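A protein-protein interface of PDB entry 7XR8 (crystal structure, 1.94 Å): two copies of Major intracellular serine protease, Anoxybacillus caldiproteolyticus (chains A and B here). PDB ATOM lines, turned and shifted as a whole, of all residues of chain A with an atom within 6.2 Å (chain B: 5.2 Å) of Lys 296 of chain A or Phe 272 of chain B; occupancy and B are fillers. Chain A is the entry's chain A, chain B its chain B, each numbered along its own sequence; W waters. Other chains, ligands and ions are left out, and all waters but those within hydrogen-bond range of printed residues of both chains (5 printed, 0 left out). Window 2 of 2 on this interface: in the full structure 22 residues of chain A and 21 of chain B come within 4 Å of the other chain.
The side-chain amide oxygen (OD1) of Asn 301 of chain A lies within hydrogen-bond range of the side-chain amide nitrogen (NE2) of Gln 284 of chain B (2.8 Å).
The side-chain carboxylate (OE1) of Glu 271 of chain B is in salt-bridge range of the side-chain amino group (NZ) of Lys 296 of chain A, at 3.7 Å.
OG of Ser 268 of chain B lies close to OE1 of Gln 284 of chain B (3.5 Å).
The backbone NH (N) of Asn 301 of chain A is in hydrogen-bond range of the backbone carbonyl oxygen (O) of Asp 227 of chain A (2.9 Å).
Among the printed residues, merely in contact across the chains: Lys 296 of chain A with Phe 272 of chain B, Gly 300 of chain A with Phe 272 of chain B and Asn 301 of chain A with Phe 272 of chain B.
Of the printed residues of chain B, Lys 296 of chain A touches Glu 271 (3.3 Å) and Phe 272 (3.9 Å).
Printed residues of chain B within 4 Å of Gly 300 of chain A: Phe 272 (3.99 Å).
Printed residues of chain B within 4 Å of Asn 301 of chain A: Phe 272 (3.7 Å) and Gln 284 (2.8 Å).
Of the printed residues of chain A, Glu 271 of chain B touches Lys 296.
Printed residues of chain A within 4 Å of Phe 272 of chain B: Lys 296, Gly 300 and Asn 301.
Glu 273 of chain B touches none of the printed residues of chain A.
Arg 274 of chain B touches none of the printed residues of chain A.
Of the printed residues of chain A, Gln 284 of chain B touches Asn 301 (2.8 Å).
The nearest printed residue of chain B that does not touch Lys 296 of chain A is Ser 268 of chain B (5.8 Å).
The nearest printed residue of chain A that does not touch Phe 272 of chain B is Ile 226 of chain A (4.2 Å).
Of the 10 printed residues of chain B, 3 touch a printed residue of chain A.
Among the printed residues, 5 pairs touch across the chains.
No position is printed for both chains.
Of the 5 pairs that touch across the chains among the printed residues, none has its exchanged pair printed and touching as well.
Water W4 bridges OE1 of Gln 284 of chain B (2.7 Å) and OD1 of Asn 301 of chain A (3.4 Å).
Water W1 lies within hydrogen-bond range of the backbone carbonyl oxygen of Glu 271 of chain B (2.7 Å), the backbone NH of Ala 297 of chain A (3.1 Å) and the backbone NH of Lys 296 of chain A (3.2 Å).
Water W2 bridges OD1 of Asp 227 of chain A (2.7 Å) and NH2 of Arg 274 of chain B (3.1 Å).
Water W3 lies within hydrogen-bond range of the backbone NH of Lys 296 of chain A (2.8 Å) and the backbone carbonyl oxygen of Glu 271 of chain B (3.2 Å).
Water W5 bridges the side-chain amide nitrogen of Asn 301 of chain A and the side-chain amide nitrogen of Gln 284 of chain B.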
ATOM      1  N   ILE A 226       9.769   9.986 -24.685  1.00  0.00           N
ATOM      2  CA  ILE A 226       9.788  10.288 -26.103  1.00  0.00           C
ATOM      3  C   ILE A 226      10.360   9.099 -26.855  1.00  0.00           C
ATOM      4  O   ILE A 226      11.107   8.268 -26.318  1.00  0.00           O
ATOM      5  CB  ILE A 226      10.601  11.566 -26.410  1.00  0.00           C
ATOM      6  CG1 ILE A 226      12.042  11.400 -25.925  1.00  0.00           C
ATOM      7  CG2 ILE A 226       9.944  12.811 -25.780  1.00  0.00           C
ATOM      8  CD1 ILE A 226      12.903  12.612 -26.159  1.00  0.00           C
ATOM      9  N   ASP A 227      10.033   9.030 -28.136  1.00  0.00           N
ATOM     10  CA  ASP A 227      10.581   7.957 -28.953  1.00  0.00           C
ATOM     11  C   ASP A 227      11.870   8.374 -29.647  1.00  0.00           C
ATOM     12  O   ASP A 227      12.821   7.587 -29.708  1.00  0.00           O
ATOM     13  CB  ASP A 227       9.533   7.498 -29.974  1.00  0.00           C
ATOM     14  CG  ASP A 227       8.363   6.782 -29.320  1.00  0.00           C
ATOM     15  OD1 ASP A 227       8.561   5.645 -28.842  1.00  0.00           O
ATOM     16  OD2 ASP A 227       7.253   7.362 -29.260  1.00  0.00           O
ATOM     17  N   PRO A 291      22.100   7.374 -31.685  1.00  0.00           N
ATOM     18  CA  PRO A 291      22.248   7.707 -30.261  1.00  0.00           C
ATOM     19  C   PRO A 291      23.195   8.883 -30.108  1.00  0.00           C
ATOM     20  O   PRO A 291      24.177   9.001 -30.842  1.00  0.00           O
ATOM     21  CB  PRO A 291      22.843   6.434 -29.643  1.00  0.00           C
ATOM     22  CG  PRO A 291      22.571   5.339 -30.653  1.00  0.00           C
ATOM     23  CD  PRO A 291      22.605   6.026 -31.994  1.00  0.00           C
ATOM     24  N   PHE A 294      23.142  10.747 -24.552  1.00  0.00           N
ATOM     25  CA  PHE A 294      22.312  11.166 -23.439  1.00  0.00           C
ATOM     26  C   PHE A 294      21.514   9.985 -22.911  1.00  0.00           C
ATOM     27  O   PHE A 294      21.395   8.957 -23.587  1.00  0.00           O
ATOM     28  CB  PHE A 294      21.383  12.284 -23.890  1.00  0.00           C
ATOM     29  CG  PHE A 294      22.113  13.479 -24.423  1.00  0.00           C
ATOM     30  CD1 PHE A 294      22.885  14.259 -23.581  1.00  0.00           C
ATOM     31  CD2 PHE A 294      22.052  13.807 -25.769  1.00  0.00           C
ATOM     32  CE1 PHE A 294      23.556  15.367 -24.062  1.00  0.00           C
ATOM     33  CE2 PHE A 294      22.736  14.910 -26.263  1.00  0.00           C
ATOM     34  CZ  PHE A 294      23.489  15.691 -25.406  1.00  0.00           C
ATOM     35  N   PRO A 295      20.966  10.082 -21.696  1.00  0.00           N
ATOM     36  CA  PRO A 295      20.090   9.010 -21.210  1.00  0.00           C
ATOM     37  C   PRO A 295      18.832   8.915 -22.062  1.00  0.00           C
ATOM     38  O   PRO A 295      18.400   9.892 -22.675  1.00  0.00           O
ATOM     39  CB  PRO A 295      19.767   9.432 -19.769  1.00  0.00           C
ATOM     40  CG  PRO A 295      20.840  10.393 -19.394  1.00  0.00           C
ATOM     41  CD  PRO A 295      21.212  11.100 -20.659  1.00  0.00           C
ATOM     42  N   LYS A 296      18.257   7.709 -22.111  1.00  0.00           N
ATOM     43  CA  LYS A 296      17.083   7.484 -22.955  1.00  0.00           C
ATOM     44  C   LYS A 296      15.895   8.316 -22.504  1.00  0.00           C
ATOM     45  O   LYS A 296      15.033   8.663 -23.320  1.00  0.00           O
ATOM     46  CB  LYS A 296      16.717   6.001 -22.972  1.00  0.00           C
ATOM     47  CG  LYS A 296      17.891   5.124 -23.260  1.00  0.00           C
ATOM     48  CD  LYS A 296      18.258   5.214 -24.708  1.00  0.00           C
ATOM     49  CE  LYS A 296      19.159   4.066 -25.123  1.00  0.00           C
ATOM     50  NZ  LYS A 296      20.540   4.526 -25.419  1.00  0.00           N
ATOM     51  N   ALA A 297      15.836   8.668 -21.218  1.00  0.00           N
ATOM     52  CA  ALA A 297      14.782   9.556 -20.747  1.00  0.00           C
ATOM     53  C   ALA A 297      14.908  10.959 -21.317  1.00  0.00           C
ATOM     54  O   ALA A 297      13.984  11.765 -21.153  1.00  0.00           O
ATOM     55  CB  ALA A 297      14.785   9.605 -19.217  1.00  0.00           C
ATOM     56  N   LEU A 298      16.017  11.270 -21.980  1.00  0.00           N
ATOM     57  CA  LEU A 298      16.237  12.566 -22.604  1.00  0.00           C
ATOM     58  C   LEU A 298      16.258  12.516 -24.123  1.00  0.00           C
ATOM     59  O   LEU A 298      15.711  13.410 -24.767  1.00  0.00           O
ATOM     60  CB  LEU A 298      17.553  13.170 -22.114  1.00  0.00           C
ATOM     61  CG  LEU A 298      17.504  13.750 -20.700  1.00  0.00           C
ATOM     62  CD1 LEU A 298      18.854  14.351 -20.364  1.00  0.00           C
ATOM     63  CD2 LEU A 298      16.393  14.784 -20.585  1.00  0.00           C
ATOM     64  N   GLU A 299      16.898  11.520 -24.730  1.00  0.00           N
ATOM     65  CA  GLU A 299      16.953  11.457 -26.186  1.00  0.00           C
ATOM     66  C   GLU A 299      16.085  10.354 -26.766  1.00  0.00           C
ATOM     67  O   GLU A 299      16.005  10.237 -27.989  1.00  0.00           O
ATOM     68  CB  GLU A 299      18.395  11.272 -26.666  1.00  0.00           C
ATOM     69  CG  GLU A 299      18.958   9.908 -26.357  1.00  0.00           C
ATOM     70  CD  GLU A 299      20.352   9.715 -26.908  1.00  0.00           C
ATOM     71  OE1 GLU A 299      21.190  10.627 -26.743  1.00  0.00           O
ATOM     72  OE2 GLU A 299      20.607   8.652 -27.512  1.00  0.00           O
ATOM     73  N   GLY A 300      15.424   9.573 -25.931  1.00  0.00           N
ATOM     74  CA  GLY A 300      14.730   8.396 -26.427  1.00  0.00           C
ATOM     75  C   GLY A 300      15.715   7.522 -27.174  1.00  0.00           C
ATOM     76  O   GLY A 300      16.788   7.186 -26.658  1.00  0.00           O
ATOM     77  N   ASN A 301      15.368   7.197 -28.414  1.00  0.00           N
ATOM     78  CA  ASN A 301      16.184   6.356 -29.273  1.00  0.00           C
ATOM     79  C   ASN A 301      17.261   7.130 -30.000  1.00  0.00           C
ATOM     80  O   ASN A 301      18.067   6.526 -30.720  1.00  0.00           O
ATOM     81  CB  ASN A 301      15.285   5.631 -30.273  1.00  0.00           C
ATOM     82  CG  ASN A 301      14.556   4.502 -29.626  1.00  0.00           C
ATOM     83  OD1 ASN A 301      15.189   3.543 -29.191  1.00  0.00           O
ATOM     84  ND2 ASN A 301      13.225   4.614 -29.509  1.00  0.00           N
ATOM     85  N   GLY A 302      17.305   8.437 -29.825  1.00  0.00           N
ATOM     86  CA  GLY A 302      18.313   9.252 -30.460  1.00  0.00           C
ATOM     87  C   GLY A 302      17.736  10.127 -31.558  1.00  0.00           C
ATOM     88  O   GLY A 302      16.518  10.260 -31.734  1.00  0.00           O
ATOM     89  N   LEU B 267      18.223  -4.636 -21.157  1.00  0.00           N
ATOM     90  CA  LEU B 267      18.934  -3.395 -21.453  1.00  0.00           C
ATOM     91  C   LEU B 267      17.966  -2.227 -21.614  1.00  0.00           C
ATOM     92  O   LEU B 267      18.112  -1.182 -20.971  1.00  0.00           O
ATOM     93  CB  LEU B 267      19.769  -3.582 -22.724  1.00  0.00           C
ATOM     94  CG  LEU B 267      20.479  -2.361 -23.312  1.00  0.00           C
ATOM     95  CD1 LEU B 267      21.431  -1.746 -22.301  1.00  0.00           C
ATOM     96  CD2 LEU B 267      21.220  -2.733 -24.605  1.00  0.00           C
ATOM     97  N   SER B 268      16.957  -2.395 -22.460  1.00  0.00           N
ATOM     98  CA  SER B 268      16.117  -1.260 -22.826  1.00  0.00           C
ATOM     99  C   SER B 268      15.226  -0.818 -21.673  1.00  0.00           C
ATOM    100  O   SER B 268      15.038   0.386 -21.458  1.00  0.00           O
ATOM    101  CB  SER B 268      15.287  -1.609 -24.058  1.00  0.00           C
ATOM    102  OG  SER B 268      16.138  -1.664 -25.183  1.00  0.00           O
ATOM    103  N   GLU B 269      14.658  -1.760 -20.923  1.00  0.00           N
ATOM    104  CA  GLU B 269      13.817  -1.332 -19.806  1.00  0.00           C
ATOM    105  C   GLU B 269      14.654  -0.642 -18.736  1.00  0.00           C
ATOM    106  O   GLU B 269      14.186   0.308 -18.097  1.00  0.00           O
ATOM    107  CB  GLU B 269      13.021  -2.515 -19.250  1.00  0.00           C
ATOM    108  CG  GLU B 269      11.989  -3.031 -20.286  1.00  0.00           C
ATOM    109  CD  GLU B 269      10.919  -3.963 -19.717  1.00  0.00           C
ATOM    110  OE1 GLU B 269      11.214  -4.743 -18.787  1.00  0.00           O
ATOM    111  OE2 GLU B 269       9.773  -3.922 -20.215  1.00  0.00           O
ATOM    112  N   LYS B 270      15.906  -1.064 -18.580  1.00  0.00           N
ATOM    113  CA  LYS B 270      16.826  -0.389 -17.668  1.00  0.00           C
ATOM    114  C   LYS B 270      17.114   1.035 -18.129  1.00  0.00           C
ATOM    115  O   LYS B 270      17.016   1.982 -17.341  1.00  0.00           O
ATOM    116  CB  LYS B 270      18.120  -1.197 -17.559  1.00  0.00           C
ATOM    117  CG  LYS B 270      19.191  -0.607 -16.640  1.00  0.00           C
ATOM    118  CD  LYS B 270      20.516  -1.356 -16.823  1.00  0.00           C
ATOM    119  CE  LYS B 270      21.480  -1.100 -15.687  1.00  0.00           C
ATOM    120  NZ  LYS B 270      21.871   0.340 -15.648  1.00  0.00           N
ATOM    121  N   GLU B 271      17.460   1.209 -19.409  1.00  0.00           N
ATOM    122  CA  GLU B 271      17.881   2.523 -19.894  1.00  0.00           C
ATOM    123  C   GLU B 271      16.695   3.468 -20.080  1.00  0.00           C
ATOM    124  O   GLU B 271      16.811   4.667 -19.814  1.00  0.00           O
ATOM    125  CB  GLU B 271      18.666   2.370 -21.205  1.00  0.00           C
ATOM    126  CG  GLU B 271      19.982   1.599 -21.046  1.00  0.00           C
ATOM    127  CD  GLU B 271      20.857   1.616 -22.291  1.00  0.00           C
ATOM    128  OE1 GLU B 271      20.330   1.472 -23.417  1.00  0.00           O
ATOM    129  OE2 GLU B 271      22.091   1.775 -22.144  1.00  0.00           O
ATOM    130  N   PHE B 272      15.553   2.958 -20.551  1.00  0.00           N
ATOM    131  CA  PHE B 272      14.345   3.766 -20.634  1.00  0.00           C
ATOM    132  C   PHE B 272      13.675   3.962 -19.281  1.00  0.00           C
ATOM    133  O   PHE B 272      12.781   4.806 -19.171  1.00  0.00           O
ATOM    134  CB  PHE B 272      13.344   3.140 -21.609  1.00  0.00           C
ATOM    135  CG  PHE B 272      13.618   3.479 -23.052  1.00  0.00           C
ATOM    136  CD1 PHE B 272      13.089   4.636 -23.620  1.00  0.00           C
ATOM    137  CD2 PHE B 272      14.415   2.656 -23.828  1.00  0.00           C
ATOM    138  CE1 PHE B 272      13.348   4.955 -24.943  1.00  0.00           C
ATOM    139  CE2 PHE B 272      14.681   2.970 -25.156  1.00  0.00           C
ATOM    140  CZ  PHE B 272      14.144   4.114 -25.713  1.00  0.00           C
ATOM    141  N   GLU B 273      14.067   3.184 -18.274  1.00  0.00           N
ATOM    142  CA  GLU B 273      13.574   3.311 -16.901  1.00  0.00           C
ATOM    143  C   GLU B 273      12.062   3.102 -16.813  1.00  0.00           C
ATOM    144  O   GLU B 273      11.350   3.849 -16.141  1.00  0.00           O
ATOM    145  CB  GLU B 273      13.984   4.661 -16.301  1.00  0.00           C
ATOM    146  CG  GLU B 273      15.489   4.893 -16.340  1.00  0.00           C
ATOM    147  CD  GLU B 273      15.922   6.189 -15.660  1.00  0.00           C
ATOM    148  OE1 GLU B 273      15.071   7.083 -15.463  1.00  0.00           O
ATOM    149  OE2 GLU B 273      17.122   6.313 -15.324  1.00  0.00           O
ATOM    150  N   ARG B 274      11.576   2.049 -17.471  1.00  0.00           N
ATOM    151  CA  ARG B 274      10.149   1.729 -17.509  1.00  0.00           C
ATOM    152  C   ARG B 274       9.942   0.445 -18.301  1.00  0.00           C
ATOM    153  O   ARG B 274      10.791   0.049 -19.101  1.00  0.00           O
ATOM    154  CB  ARG B 274       9.323   2.865 -18.136  1.00  0.00           C
ATOM    155  CG  ARG B 274       9.553   3.089 -19.625  1.00  0.00           C
ATOM    156  CD  ARG B 274       8.478   4.013 -20.182  1.00  0.00           C
ATOM    157  NE  ARG B 274       8.434   4.046 -21.638  1.00  0.00           N
ATOM    158  CZ  ARG B 274       9.145   4.882 -22.388  1.00  0.00           C
ATOM    159  NH1 ARG B 274       9.976   5.748 -21.821  1.00  0.00           N
ATOM    160  NH2 ARG B 274       9.026   4.846 -23.709  1.00  0.00           N
ATOM    161  N   LEU B 276       8.599  -1.587 -21.310  1.00  0.00           N
ATOM    162  CA  LEU B 276       8.382  -1.279 -22.721  1.00  0.00           C
ATOM    163  C   LEU B 276       7.312  -2.204 -23.299  1.00  0.00           C
ATOM    164  O   LEU B 276       7.205  -3.365 -22.903  1.00  0.00           O
ATOM    165  CB  LEU B 276       9.692  -1.432 -23.510  1.00  0.00           C
ATOM    166  CG  LEU B 276      10.678  -0.260 -23.532  1.00  0.00           C
ATOM    167  CD1 LEU B 276      11.209   0.028 -22.156  1.00  0.00           C
ATOM    168  CD2 LEU B 276      11.838  -0.498 -24.499  1.00  0.00           C
ATOM    169  N   GLN B 284      13.268  -2.102 -30.712  1.00  0.00           N
ATOM    170  CA  GLN B 284      14.609  -2.214 -30.138  1.00  0.00           C
ATOM    171  C   GLN B 284      15.391  -3.354 -30.797  1.00  0.00           C
ATOM    172  O   GLN B 284      16.611  -3.261 -30.965  1.00  0.00           O
ATOM    173  CB  GLN B 284      14.532  -2.416 -28.619  1.00  0.00           C
ATOM    174  CG  GLN B 284      13.951  -1.225 -27.845  1.00  0.00           C
ATOM    175  CD  GLN B 284      14.687   0.066 -28.162  1.00  0.00           C
ATOM    176  OE1 GLN B 284      15.917   0.105 -28.172  1.00  0.00           O
ATOM    177  NE2 GLN B 284      13.935   1.121 -28.452  1.00  0.00           N
HETATM  178  O   HOH W   1      17.530   7.146 -19.057  1.00  0.00           O
HETATM  179  O   HOH W   2       9.734   4.406 -26.734  1.00  0.00           O
HETATM  180  O   HOH W   3      19.708   5.779 -20.614  1.00  0.00           O
HETATM  181  O   HOH W   4      17.753   1.934 -27.575  1.00  0.00           O
HETATM  182  O   HOH W   5      11.076   2.548 -28.429  1.00  0.00           O
